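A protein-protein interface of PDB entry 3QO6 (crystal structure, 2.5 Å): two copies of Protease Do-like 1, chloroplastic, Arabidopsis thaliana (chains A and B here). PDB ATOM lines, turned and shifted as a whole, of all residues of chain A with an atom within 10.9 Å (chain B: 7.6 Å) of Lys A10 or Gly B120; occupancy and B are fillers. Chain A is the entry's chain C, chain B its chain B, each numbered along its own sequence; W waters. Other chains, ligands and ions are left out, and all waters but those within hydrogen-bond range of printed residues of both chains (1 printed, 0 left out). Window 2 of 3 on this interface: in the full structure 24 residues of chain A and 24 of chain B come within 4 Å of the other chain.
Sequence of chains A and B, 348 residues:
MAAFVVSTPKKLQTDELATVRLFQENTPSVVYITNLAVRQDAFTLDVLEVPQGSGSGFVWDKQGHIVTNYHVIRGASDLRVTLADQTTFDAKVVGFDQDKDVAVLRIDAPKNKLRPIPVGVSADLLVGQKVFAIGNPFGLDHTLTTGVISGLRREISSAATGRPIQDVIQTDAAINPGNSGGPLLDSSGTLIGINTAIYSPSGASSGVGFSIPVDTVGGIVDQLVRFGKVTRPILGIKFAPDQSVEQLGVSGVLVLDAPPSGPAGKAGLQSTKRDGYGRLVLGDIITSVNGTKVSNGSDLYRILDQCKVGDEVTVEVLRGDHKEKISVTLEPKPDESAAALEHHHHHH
The side-chain carboxylate (OD1) of Asp B186 lies within salt-bridge range of the side-chain amino group (NZ) of Lys A10 (3.5 Å).
The side-chain hydroxyl (OG) of Ser B187 lies within hydrogen-bond range of the side-chain carboxylate (OE1) of Glu A16 (2.5 Å).
The backbone nitrogen (N) of Pro A9 lies close to the side-chain carboxylate (OD2) of Asp B124 (3.4 Å).
Ser A7 touches Asp B124 (O to OD2, 3.6 Å).
OD2 of Asp B124 touches C of Thr A8, 3.4 Å away.
NZ of Lys A10 touches CA of Gly B120, at 3.3 Å.
Lys A10 touches Val B121.
OG of Ser B188 touches CD of Lys A10, at 3.4 Å.
Lys A10 touches Thr B190 (NZ to CG2, 3.0 Å).
Gln B129 touches Leu A12.
Glu A16 touches Gln B129.
Val A20 touches Gln B129.
Printed residues of chain A that touch a printed residue of chain B: Ser A7, Thr A8, Pro A9, Lys A10, Leu A12, Glu A16 and Val A20.
Of the 23 printed residues of chain B, 8 touch a printed residue of chain A.
Printed residues of chain B that touch a printed residue of chain A: Gly B120, Val B121, Asp B124, Gln B129, Asp B186, Ser B187, Ser B188 and Thr B190.
Among the printed residues, 12 pairs touch across the chains.
Printed residues of chain B within 4 Å of Lys A10: Gly B120, Val B121, Asp B186, Ser B188 and Thr B190.
Of chain A, only Lys A10 (3.3 Å) comes within 4 Å of Gly B120.
No residue of chain A comes within 4 Å of Val B119.
Of chain A, only Lys A10 comes within 4 Å of Thr B190.
No residue of chain A comes within 4 Å of Val B214.
Printed residues of chain A within 4 Å of Gln B129: Leu A12 (3.7 Å), Glu A16 (3.2 Å) and Val A20 (3.5 Å).
Of the printed residues of chain B, Leu A12 touches Gln B129 (3.7 Å).
Ser B122 touches none of the printed residues of chain A.
Ile B192 touches none of the printed residues of chain A.
The nearest residue of chain B that does not touch Lys A10 is Val B119 (4.9 Å).
The nearest residue of chain A that does not touch Gly B120 is Ser A7 (7.9 Å).
Water W1 lies within hydrogen-bond range of the side-chain amide nitrogen (NE2) of Gln B129, the side-chain carboxylate (OE2) of Glu A16 and the backbone NH (N) of Ser B187.
No position is printed for both chains.
Of the 12 pairs that touch across the chains among the printed residues, none has its exchanged pair printed and touching as well.
The backbone NH of Gly B120 lies within hydrogen-bond range of the backbone carbonyl oxygen of Leu B191 (3.0 Å).
OE1 of Gln B129 lies within hydrogen-bond range of N of Leu B126.
N of Ser B188 is in hydrogen-bond range of OD2 of Asp B186 (2.7 Å).
OD2 of Asp B186 is in hydrogen-bond range of N of Gly B189 (3.4 Å).
The backbone NH (N) of Thr B190 sits at hydrogen-bond distance from the side-chain carboxylate (OD2) of Asp B186, at 3.4 Å.
The backbone NH of Gln A13 lies within hydrogen-bond range of the side-chain carboxylate of Glu A16 (3.0 Å).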
ATOM      1  N   SER A   7      -3.127 -41.399  -2.267  1.00  0.00           N
ATOM      2  CA  SER A   7      -3.438 -39.949  -2.453  1.00  0.00           C
ATOM      3  C   SER A   7      -4.336 -39.693  -3.671  1.00  0.00           C
ATOM      4  O   SER A   7      -4.100 -40.226  -4.762  1.00  0.00           O
ATOM      5  CB  SER A   7      -2.130 -39.143  -2.571  1.00  0.00           C
ATOM      6  OG  SER A   7      -1.204 -39.755  -3.458  1.00  0.00           O
ATOM      7  N   THR A   8      -5.374 -38.883  -3.468  1.00  0.00           N
ATOM      8  CA  THR A   8      -6.323 -38.534  -4.531  1.00  0.00           C
ATOM      9  C   THR A   8      -6.085 -37.087  -5.014  1.00  0.00           C
ATOM     10  O   THR A   8      -5.919 -36.177  -4.196  1.00  0.00           O
ATOM     11  CB  THR A   8      -7.802 -38.671  -4.031  1.00  0.00           C
ATOM     12  OG1 THR A   8      -8.069 -37.686  -3.019  1.00  0.00           O
ATOM     13  CG2 THR A   8      -8.049 -40.070  -3.449  1.00  0.00           C
ATOM     14  N   PRO A   9      -6.062 -36.861  -6.347  1.00  0.00           N
ATOM     15  CA  PRO A   9      -5.841 -35.515  -6.900  1.00  0.00           C
ATOM     16  C   PRO A   9      -6.829 -34.473  -6.360  1.00  0.00           C
ATOM     17  O   PRO A   9      -7.972 -34.807  -6.037  1.00  0.00           O
ATOM     18  CB  PRO A   9      -5.997 -35.730  -8.408  1.00  0.00           C
ATOM     19  CG  PRO A   9      -5.520 -37.126  -8.596  1.00  0.00           C
ATOM     20  CD  PRO A   9      -6.171 -37.853  -7.431  1.00  0.00           C
ATOM     21  N   LYS A  10      -6.382 -33.216  -6.261  1.00  0.00           N
ATOM     22  CA  LYS A  10      -7.228 -32.123  -5.759  1.00  0.00           C
ATOM     23  C   LYS A  10      -8.037 -31.508  -6.899  1.00  0.00           C
ATOM     24  O   LYS A  10      -7.546 -31.405  -8.031  1.00  0.00           O
ATOM     25  CB  LYS A  10      -6.362 -31.052  -5.072  1.00  0.00           C
ATOM     26  CG  LYS A  10      -5.699 -31.556  -3.796  1.00  0.00           C
ATOM     27  CD  LYS A  10      -4.725 -30.568  -3.208  1.00  0.00           C
ATOM     28  CE  LYS A  10      -3.841 -31.233  -2.143  1.00  0.00           C
ATOM     29  NZ  LYS A  10      -2.469 -30.615  -2.086  1.00  0.00           N
ATOM     30  N   LYS A  11      -9.278 -31.115  -6.607  1.00  0.00           N
ATOM     31  CA  LYS A  11     -10.147 -30.518  -7.624  1.00  0.00           C
ATOM     32  C   LYS A  11      -9.462 -29.283  -8.203  1.00  0.00           C
ATOM     33  O   LYS A  11      -9.068 -28.392  -7.450  1.00  0.00           O
ATOM     34  CB  LYS A  11     -11.487 -30.098  -7.006  1.00  0.00           C
ATOM     35  CG  LYS A  11     -12.694 -30.158  -7.956  1.00  0.00           C
ATOM     36  CD  LYS A  11     -13.235 -31.602  -8.071  1.00  0.00           C
ATOM     37  CE  LYS A  11     -14.581 -31.671  -8.823  1.00  0.00           C
ATOM     38  NZ  LYS A  11     -15.244 -33.023  -8.794  1.00  0.00           N
ATOM     39  N   LEU A  12      -9.307 -29.232  -9.524  1.00  0.00           N
ATOM     40  CA  LEU A  12      -8.680 -28.078 -10.146  1.00  0.00           C
ATOM     41  C   LEU A  12      -9.746 -27.109 -10.632  1.00  0.00           C
ATOM     42  O   LEU A  12     -10.881 -27.498 -10.898  1.00  0.00           O
ATOM     43  CB  LEU A  12      -7.831 -28.503 -11.329  1.00  0.00           C
ATOM     44  CG  LEU A  12      -6.726 -29.511 -11.055  1.00  0.00           C
ATOM     45  CD1 LEU A  12      -5.996 -29.788 -12.355  1.00  0.00           C
ATOM     46  CD2 LEU A  12      -5.769 -28.989  -9.984  1.00  0.00           C
ATOM     47  N   GLN A  13      -9.382 -25.840 -10.736  1.00  0.00           N
ATOM     48  CA  GLN A  13     -10.296 -24.815 -11.226  1.00  0.00           C
ATOM     49  C   GLN A  13     -10.571 -25.078 -12.711  1.00  0.00           C
ATOM     50  O   GLN A  13      -9.755 -25.725 -13.397  1.00  0.00           O
ATOM     51  CB  GLN A  13      -9.667 -23.446 -11.017  1.00  0.00           C
ATOM     52  CG  GLN A  13      -9.438 -23.176  -9.575  1.00  0.00           C
ATOM     53  CD  GLN A  13     -10.722 -23.364  -8.821  1.00  0.00           C
ATOM     54  OE1 GLN A  13     -11.755 -22.791  -9.197  1.00  0.00           O
ATOM     55  NE2 GLN A  13     -10.685 -24.175  -7.762  1.00  0.00           N
ATOM     56  N   THR A  14     -11.701 -24.570 -13.212  1.00  0.00           N
ATOM     57  CA  THR A  14     -12.069 -24.843 -14.591  1.00  0.00           C
ATOM     58  C   THR A  14     -11.068 -24.317 -15.583  1.00  0.00           C
ATOM     59  O   THR A  14     -10.715 -25.004 -16.537  1.00  0.00           O
ATOM     60  CB  THR A  14     -13.485 -24.328 -14.923  1.00  0.00           C
ATOM     61  OG1 THR A  14     -13.533 -22.912 -14.760  1.00  0.00           O
ATOM     62  CG2 THR A  14     -14.534 -25.006 -13.996  1.00  0.00           C
ATOM     63  N   GLU A  16      -7.706 -23.743 -15.229  1.00  0.00           N
ATOM     64  CA  GLU A  16      -6.525 -24.596 -15.268  1.00  0.00           C
ATOM     65  C   GLU A  16      -6.804 -26.014 -15.754  1.00  0.00           C
ATOM     66  O   GLU A  16      -5.962 -26.634 -16.426  1.00  0.00           O
ATOM     67  CB  GLU A  16      -5.826 -24.643 -13.900  1.00  0.00           C
ATOM     68  CG  GLU A  16      -6.707 -24.956 -12.734  1.00  0.00           C
ATOM     69  CD  GLU A  16      -5.907 -25.325 -11.502  1.00  0.00           C
ATOM     70  OE1 GLU A  16      -6.482 -25.239 -10.401  1.00  0.00           O
ATOM     71  OE2 GLU A  16      -4.715 -25.711 -11.634  1.00  0.00           O
ATOM     72  N   LEU A  17      -7.982 -26.525 -15.416  1.00  0.00           N
ATOM     73  CA  LEU A  17      -8.353 -27.871 -15.825  1.00  0.00           C
ATOM     74  C   LEU A  17      -8.340 -27.965 -17.348  1.00  0.00           C
ATOM     75  O   LEU A  17      -7.948 -28.984 -17.925  1.00  0.00           O
ATOM     76  CB  LEU A  17      -9.738 -28.214 -15.291  1.00  0.00           C
ATOM     77  CG  LEU A  17     -10.193 -29.628 -15.643  1.00  0.00           C
ATOM     78  CD1 LEU A  17      -9.302 -30.677 -14.981  1.00  0.00           C
ATOM     79  CD2 LEU A  17     -11.621 -29.768 -15.190  1.00  0.00           C
ATOM     80  N   VAL A  20      -4.988 -28.235 -18.653  1.00  0.00           N
ATOM     81  CA  VAL A  20      -4.554 -29.616 -18.417  1.00  0.00           C
ATOM     82  C   VAL A  20      -5.110 -30.561 -19.505  1.00  0.00           C
ATOM     83  O   VAL A  20      -4.396 -31.447 -19.965  1.00  0.00           O
ATOM     84  CB  VAL A  20      -4.956 -30.133 -16.984  1.00  0.00           C
ATOM     85  CG1 VAL A  20      -5.001 -31.667 -16.945  1.00  0.00           C
ATOM     86  CG2 VAL A  20      -3.926 -29.665 -15.963  1.00  0.00           C
ATOM     87  N   TRP B  60       7.888 -24.475   8.553  1.00  0.00           N
ATOM     88  CA  TRP B  60       7.440 -25.841   8.446  1.00  0.00           C
ATOM     89  C   TRP B  60       6.513 -26.298   9.548  1.00  0.00           C
ATOM     90  O   TRP B  60       5.618 -27.099   9.302  1.00  0.00           O
ATOM     91  CB  TRP B  60       8.625 -26.771   8.383  1.00  0.00           C
ATOM     92  CG  TRP B  60       8.207 -28.152   8.153  1.00  0.00           C
ATOM     93  CD1 TRP B  60       8.142 -29.140   9.076  1.00  0.00           C
ATOM     94  CD2 TRP B  60       7.810 -28.735   6.899  1.00  0.00           C
ATOM     95  NE1 TRP B  60       7.737 -30.314   8.484  1.00  0.00           N
ATOM     96  CE2 TRP B  60       7.523 -30.097   7.147  1.00  0.00           C
ATOM     97  CE3 TRP B  60       7.672 -28.244   5.586  1.00  0.00           C
ATOM     98  CZ2 TRP B  60       7.106 -30.983   6.128  1.00  0.00           C
ATOM     99  CZ3 TRP B  60       7.258 -29.130   4.573  1.00  0.00           C
ATOM    100  CH2 TRP B  60       6.980 -30.481   4.855  1.00  0.00           C
ATOM    101  N   ILE B 117       3.186 -23.722   6.276  1.00  0.00           N
ATOM    102  CA  ILE B 117       2.453 -23.857   5.014  1.00  0.00           C
ATOM    103  C   ILE B 117       1.778 -25.191   4.967  1.00  0.00           C
ATOM    104  O   ILE B 117       2.294 -26.172   5.467  1.00  0.00           O
ATOM    105  CB  ILE B 117       3.323 -23.784   3.719  1.00  0.00           C
ATOM    106  CG1 ILE B 117       4.740 -24.200   4.032  1.00  0.00           C
ATOM    107  CG2 ILE B 117       3.243 -22.415   3.082  1.00  0.00           C
ATOM    108  CD1 ILE B 117       4.832 -25.580   4.611  1.00  0.00           C
ATOM    109  N   PRO B 118       0.591 -25.231   4.374  1.00  0.00           N
ATOM    110  CA  PRO B 118      -0.159 -26.466   4.253  1.00  0.00           C
ATOM    111  C   PRO B 118       0.634 -27.333   3.299  1.00  0.00           C
ATOM    112  O   PRO B 118       0.977 -26.901   2.217  1.00  0.00           O
ATOM    113  CB  PRO B 118      -1.477 -26.000   3.655  1.00  0.00           C
ATOM    114  CG  PRO B 118      -1.611 -24.598   4.144  1.00  0.00           C
ATOM    115  CD  PRO B 118      -0.225 -24.068   3.990  1.00  0.00           C
ATOM    116  N   VAL B 119       0.939 -28.557   3.691  1.00  0.00           N
ATOM    117  CA  VAL B 119       1.718 -29.442   2.845  1.00  0.00           C
ATOM    118  C   VAL B 119       0.864 -30.170   1.824  1.00  0.00           C
ATOM    119  O   VAL B 119      -0.068 -30.842   2.187  1.00  0.00           O
ATOM    120  CB  VAL B 119       2.433 -30.474   3.705  1.00  0.00           C
ATOM    121  CG1 VAL B 119       3.013 -31.580   2.812  1.00  0.00           C
ATOM    122  CG2 VAL B 119       3.515 -29.779   4.541  1.00  0.00           C
ATOM    123  N   GLY B 120       1.182 -30.053   0.547  1.00  0.00           N
ATOM    124  CA  GLY B 120       0.388 -30.747  -0.446  1.00  0.00           C
ATOM    125  C   GLY B 120       0.981 -32.041  -0.934  1.00  0.00           C
ATOM    126  O   GLY B 120       1.852 -32.620  -0.287  1.00  0.00           O
ATOM    127  N   VAL B 121       0.509 -32.509  -2.085  1.00  0.00           N
ATOM    128  CA  VAL B 121       1.022 -33.758  -2.644  1.00  0.00           C
ATOM    129  C   VAL B 121       1.561 -33.562  -4.042  1.00  0.00           C
ATOM    130  O   VAL B 121       0.840 -33.121  -4.925  1.00  0.00           O
ATOM    131  CB  VAL B 121      -0.072 -34.846  -2.731  1.00  0.00           C
ATOM    132  CG1 VAL B 121       0.484 -36.058  -3.450  1.00  0.00           C
ATOM    133  CG2 VAL B 121      -0.530 -35.242  -1.352  1.00  0.00           C
ATOM    134  N   SER B 122       2.810 -33.934  -4.261  1.00  0.00           N
ATOM    135  CA  SER B 122       3.373 -33.757  -5.574  1.00  0.00           C
ATOM    136  C   SER B 122       3.174 -34.944  -6.484  1.00  0.00           C
ATOM    137  O   SER B 122       3.313 -34.828  -7.681  1.00  0.00           O
ATOM    138  CB  SER B 122       4.863 -33.408  -5.479  1.00  0.00           C
ATOM    139  OG  SER B 122       5.673 -34.495  -5.081  1.00  0.00           O
ATOM    140  N   ALA B 123       2.827 -36.090  -5.933  1.00  0.00           N
ATOM    141  CA  ALA B 123       2.645 -37.268  -6.776  1.00  0.00           C
ATOM    142  C   ALA B 123       1.531 -37.153  -7.806  1.00  0.00           C
ATOM    143  O   ALA B 123       1.629 -37.760  -8.847  1.00  0.00           O
ATOM    144  CB  ALA B 123       2.411 -38.493  -5.917  1.00  0.00           C
ATOM    145  N   ASP B 124       0.482 -36.382  -7.529  1.00  0.00           N
ATOM    146  CA  ASP B 124      -0.635 -36.252  -8.476  1.00  0.00           C
ATOM    147  C   ASP B 124      -0.609 -35.059  -9.441  1.00  0.00           C
ATOM    148  O   ASP B 124      -1.588 -34.801 -10.148  1.00  0.00           O
ATOM    149  CB  ASP B 124      -1.948 -36.166  -7.711  1.00  0.00           C
ATOM    150  CG  ASP B 124      -2.135 -37.303  -6.778  1.00  0.00           C
ATOM    151  OD1 ASP B 124      -1.677 -38.424  -7.117  1.00  0.00           O
ATOM    152  OD2 ASP B 124      -2.749 -37.075  -5.711  1.00  0.00           O
ATOM    153  N   LEU B 125       0.485 -34.313  -9.464  1.00  0.00           N
ATOM    154  CA  LEU B 125       0.552 -33.143 -10.315  1.00  0.00           C
ATOM    155  C   LEU B 125       0.352 -33.469 -11.804  1.00  0.00           C
ATOM    156  O   LEU B 125       0.689 -34.567 -12.281  1.00  0.00           O
ATOM    157  CB  LEU B 125       1.883 -32.407 -10.052  1.00  0.00           C
ATOM    158  CG  LEU B 125       2.065 -31.917  -8.597  1.00  0.00           C
ATOM    159  CD1 LEU B 125       3.436 -31.339  -8.402  1.00  0.00           C
ATOM    160  CD2 LEU B 125       1.011 -30.856  -8.247  1.00  0.00           C
ATOM    161  N   LEU B 126      -0.231 -32.508 -12.518  1.00  0.00           N
ATOM    162  CA  LEU B 126      -0.493 -32.623 -13.957  1.00  0.00           C
ATOM    163  C   LEU B 126       0.036 -31.395 -14.706  1.00  0.00           C
ATOM    164  O   LEU B 126      -0.225 -30.252 -14.301  1.00  0.00           O
ATOM    165  CB  LEU B 126      -1.988 -32.714 -14.192  1.00  0.00           C
ATOM    166  CG  LEU B 126      -2.668 -33.992 -13.733  1.00  0.00           C
ATOM    167  CD1 LEU B 126      -4.140 -33.710 -13.559  1.00  0.00           C
ATOM    168  CD2 LEU B 126      -2.393 -35.134 -14.752  1.00  0.00           C
ATOM    169  N   GLN B 129      -1.515 -27.431 -14.735  1.00  0.00           N
ATOM    170  CA  GLN B 129      -2.230 -26.800 -13.611  1.00  0.00           C
ATOM    171  C   GLN B 129      -1.465 -25.572 -13.147  1.00  0.00           C
ATOM    172  O   GLN B 129      -0.255 -25.502 -13.340  1.00  0.00           O
ATOM    173  CB  GLN B 129      -2.479 -27.787 -12.465  1.00  0.00           C
ATOM    174  CG  GLN B 129      -1.274 -28.357 -11.819  1.00  0.00           C
ATOM    175  CD  GLN B 129      -1.650 -29.410 -10.766  1.00  0.00           C
ATOM    176  OE1 GLN B 129      -1.515 -30.621 -11.012  1.00  0.00           O
ATOM    177  NE2 GLN B 129      -2.129 -28.954  -9.593  1.00  0.00           N
ATOM    178  N   LEU B 184       6.544 -23.303  -3.868  1.00  0.00           N
ATOM    179  CA  LEU B 184       5.766 -23.320  -5.082  1.00  0.00           C
ATOM    180  C   LEU B 184       4.430 -23.889  -4.589  1.00  0.00           C
ATOM    181  O   LEU B 184       4.384 -24.970  -4.004  1.00  0.00           O
ATOM    182  CB  LEU B 184       6.349 -24.250  -6.127  1.00  0.00           C
ATOM    183  CG  LEU B 184       5.641 -24.112  -7.491  1.00  0.00           C
ATOM    184  CD1 LEU B 184       5.880 -22.715  -8.078  1.00  0.00           C
ATOM    185  CD2 LEU B 184       6.173 -25.176  -8.431  1.00  0.00           C
ATOM    186  N   ASP B 186       0.191 -24.893  -5.333  1.00  0.00           N
ATOM    187  CA  ASP B 186      -0.750 -25.291  -6.387  1.00  0.00           C
ATOM    188  C   ASP B 186      -2.028 -24.471  -6.165  1.00  0.00           C
ATOM    189  O   ASP B 186      -2.076 -23.660  -5.221  1.00  0.00           O
ATOM    190  CB  ASP B 186      -1.019 -26.805  -6.334  1.00  0.00           C
ATOM    191  CG  ASP B 186      -1.678 -27.264  -5.024  1.00  0.00           C
ATOM    192  OD1 ASP B 186      -1.490 -28.451  -4.643  1.00  0.00           O
ATOM    193  OD2 ASP B 186      -2.386 -26.457  -4.385  1.00  0.00           O
ATOM    194  N   SER B 187      -3.057 -24.650  -6.995  1.00  0.00           N
ATOM    195  CA  SER B 187      -4.264 -23.830  -6.806  1.00  0.00           C
ATOM    196  C   SER B 187      -4.957 -23.977  -5.455  1.00  0.00           C
ATOM    197  O   SER B 187      -5.711 -23.106  -5.049  1.00  0.00           O
ATOM    198  CB  SER B 187      -5.285 -24.052  -7.926  1.00  0.00           C
ATOM    199  OG  SER B 187      -5.634 -25.409  -8.068  1.00  0.00           O
ATOM    200  N   SER B 188      -4.687 -25.066  -4.757  1.00  0.00           N
ATOM    201  CA  SER B 188      -5.289 -25.283  -3.459  1.00  0.00           C
ATOM    202  C   SER B 188      -4.577 -24.531  -2.344  1.00  0.00           C
ATOM    203  O   SER B 188      -4.945 -24.660  -1.182  1.00  0.00           O
ATOM    204  CB  SER B 188      -5.279 -26.764  -3.129  1.00  0.00           C
ATOM    205  OG  SER B 188      -5.868 -27.499  -4.177  1.00  0.00           O
ATOM    206  N   GLY B 189      -3.553 -23.760  -2.684  1.00  0.00           N
ATOM    207  CA  GLY B 189      -2.837 -23.014  -1.661  1.00  0.00           C
ATOM    208  C   GLY B 189      -2.045 -23.993  -0.833  1.00  0.00           C
ATOM    209  O   GLY B 189      -1.965 -23.898   0.380  1.00  0.00           O
ATOM    210  N   THR B 190      -1.412 -24.911  -1.540  1.00  0.00           N
ATOM    211  CA  THR B 190      -0.660 -25.983  -0.944  1.00  0.00           C
ATOM    212  C   THR B 190       0.745 -26.099  -1.487  1.00  0.00           C
ATOM    213  O   THR B 190       0.989 -25.860  -2.670  1.00  0.00           O
ATOM    214  CB  THR B 190      -1.453 -27.240  -1.191  1.00  0.00           C
ATOM    215  OG1 THR B 190      -2.276 -27.468  -0.053  1.00  0.00           O
ATOM    216  CG2 THR B 190      -0.601 -28.393  -1.489  1.00  0.00           C
ATOM    217  N   LEU B 191       1.670 -26.494  -0.620  1.00  0.00           N
ATOM    218  CA  LEU B 191       3.080 -26.607  -0.986  1.00  0.00           C
ATOM    219  C   LEU B 191       3.346 -27.788  -1.868  1.00  0.00           C
ATOM    220  O   LEU B 191       3.116 -28.914  -1.437  1.00  0.00           O
ATOM    221  CB  LEU B 191       3.941 -26.745   0.260  1.00  0.00           C
ATOM    222  CG  LEU B 191       5.404 -27.025  -0.043  1.00  0.00           C
ATOM    223  CD1 LEU B 191       6.163 -25.706  -0.212  1.00  0.00           C
ATOM    224  CD2 LEU B 191       5.987 -27.838   1.092  1.00  0.00           C
ATOM    225  N   ILE B 192       3.848 -27.562  -3.083  1.00  0.00           N
ATOM    226  CA  ILE B 192       4.115 -28.699  -3.951  1.00  0.00           C
ATOM    227  C   ILE B 192       5.565 -28.854  -4.269  1.00  0.00           C
ATOM    228  O   ILE B 192       5.973 -29.891  -4.786  1.00  0.00           O
ATOM    229  CB  ILE B 192       3.302 -28.659  -5.268  1.00  0.00           C
ATOM    230  CG1 ILE B 192       3.627 -27.387  -6.048  1.00  0.00           C
ATOM    231  CG2 ILE B 192       1.826 -28.763  -4.954  1.00  0.00           C
ATOM    232  CD1 ILE B 192       2.736 -27.176  -7.219  1.00  0.00           C
ATOM    233  N   GLY B 193       6.357 -27.839  -3.954  1.00  0.00           N
ATOM    234  CA  GLY B 193       7.785 -27.951  -4.209  1.00  0.00           C
ATOM    235  C   GLY B 193       8.543 -26.772  -3.639  1.00  0.00           C
ATOM    236  O   GLY B 193       7.914 -25.824  -3.137  1.00  0.00           O
ATOM    237  N   VAL B 214       7.590 -31.617  -3.275  1.00  0.00           N
ATOM    238  CA  VAL B 214       7.216 -31.707  -1.881  1.00  0.00           C
ATOM    239  C   VAL B 214       7.317 -33.104  -1.273  1.00  0.00           C
ATOM    240  O   VAL B 214       7.768 -33.261  -0.139  1.00  0.00           O
ATOM    241  CB  VAL B 214       5.786 -31.178  -1.708  1.00  0.00           C
ATOM    242  CG1 VAL B 214       4.823 -32.065  -2.459  1.00  0.00           C
ATOM    243  CG2 VAL B 214       5.445 -31.050  -0.241  1.00  0.00           C
ATOM    244  N   ASP B 215       6.903 -34.120  -2.014  1.00  0.00           N
ATOM    245  CA  ASP B 215       6.959 -35.467  -1.485  1.00  0.00           C
ATOM    246  C   ASP B 215       8.366 -35.860  -1.032  1.00  0.00           C
ATOM    247  O   ASP B 215       8.545 -36.396   0.073  1.00  0.00           O
ATOM    248  CB  ASP B 215       6.404 -36.473  -2.504  1.00  0.00           C
ATOM    249  CG  ASP B 215       4.888 -36.346  -2.673  1.00  0.00           C
ATOM    250  OD1 ASP B 215       4.271 -35.447  -2.031  1.00  0.00           O
ATOM    251  OD2 ASP B 215       4.313 -37.150  -3.447  1.00  0.00           O
HETATM  252  O   HOH W   1      -2.834 -26.252  -9.621  1.00  0.00           O
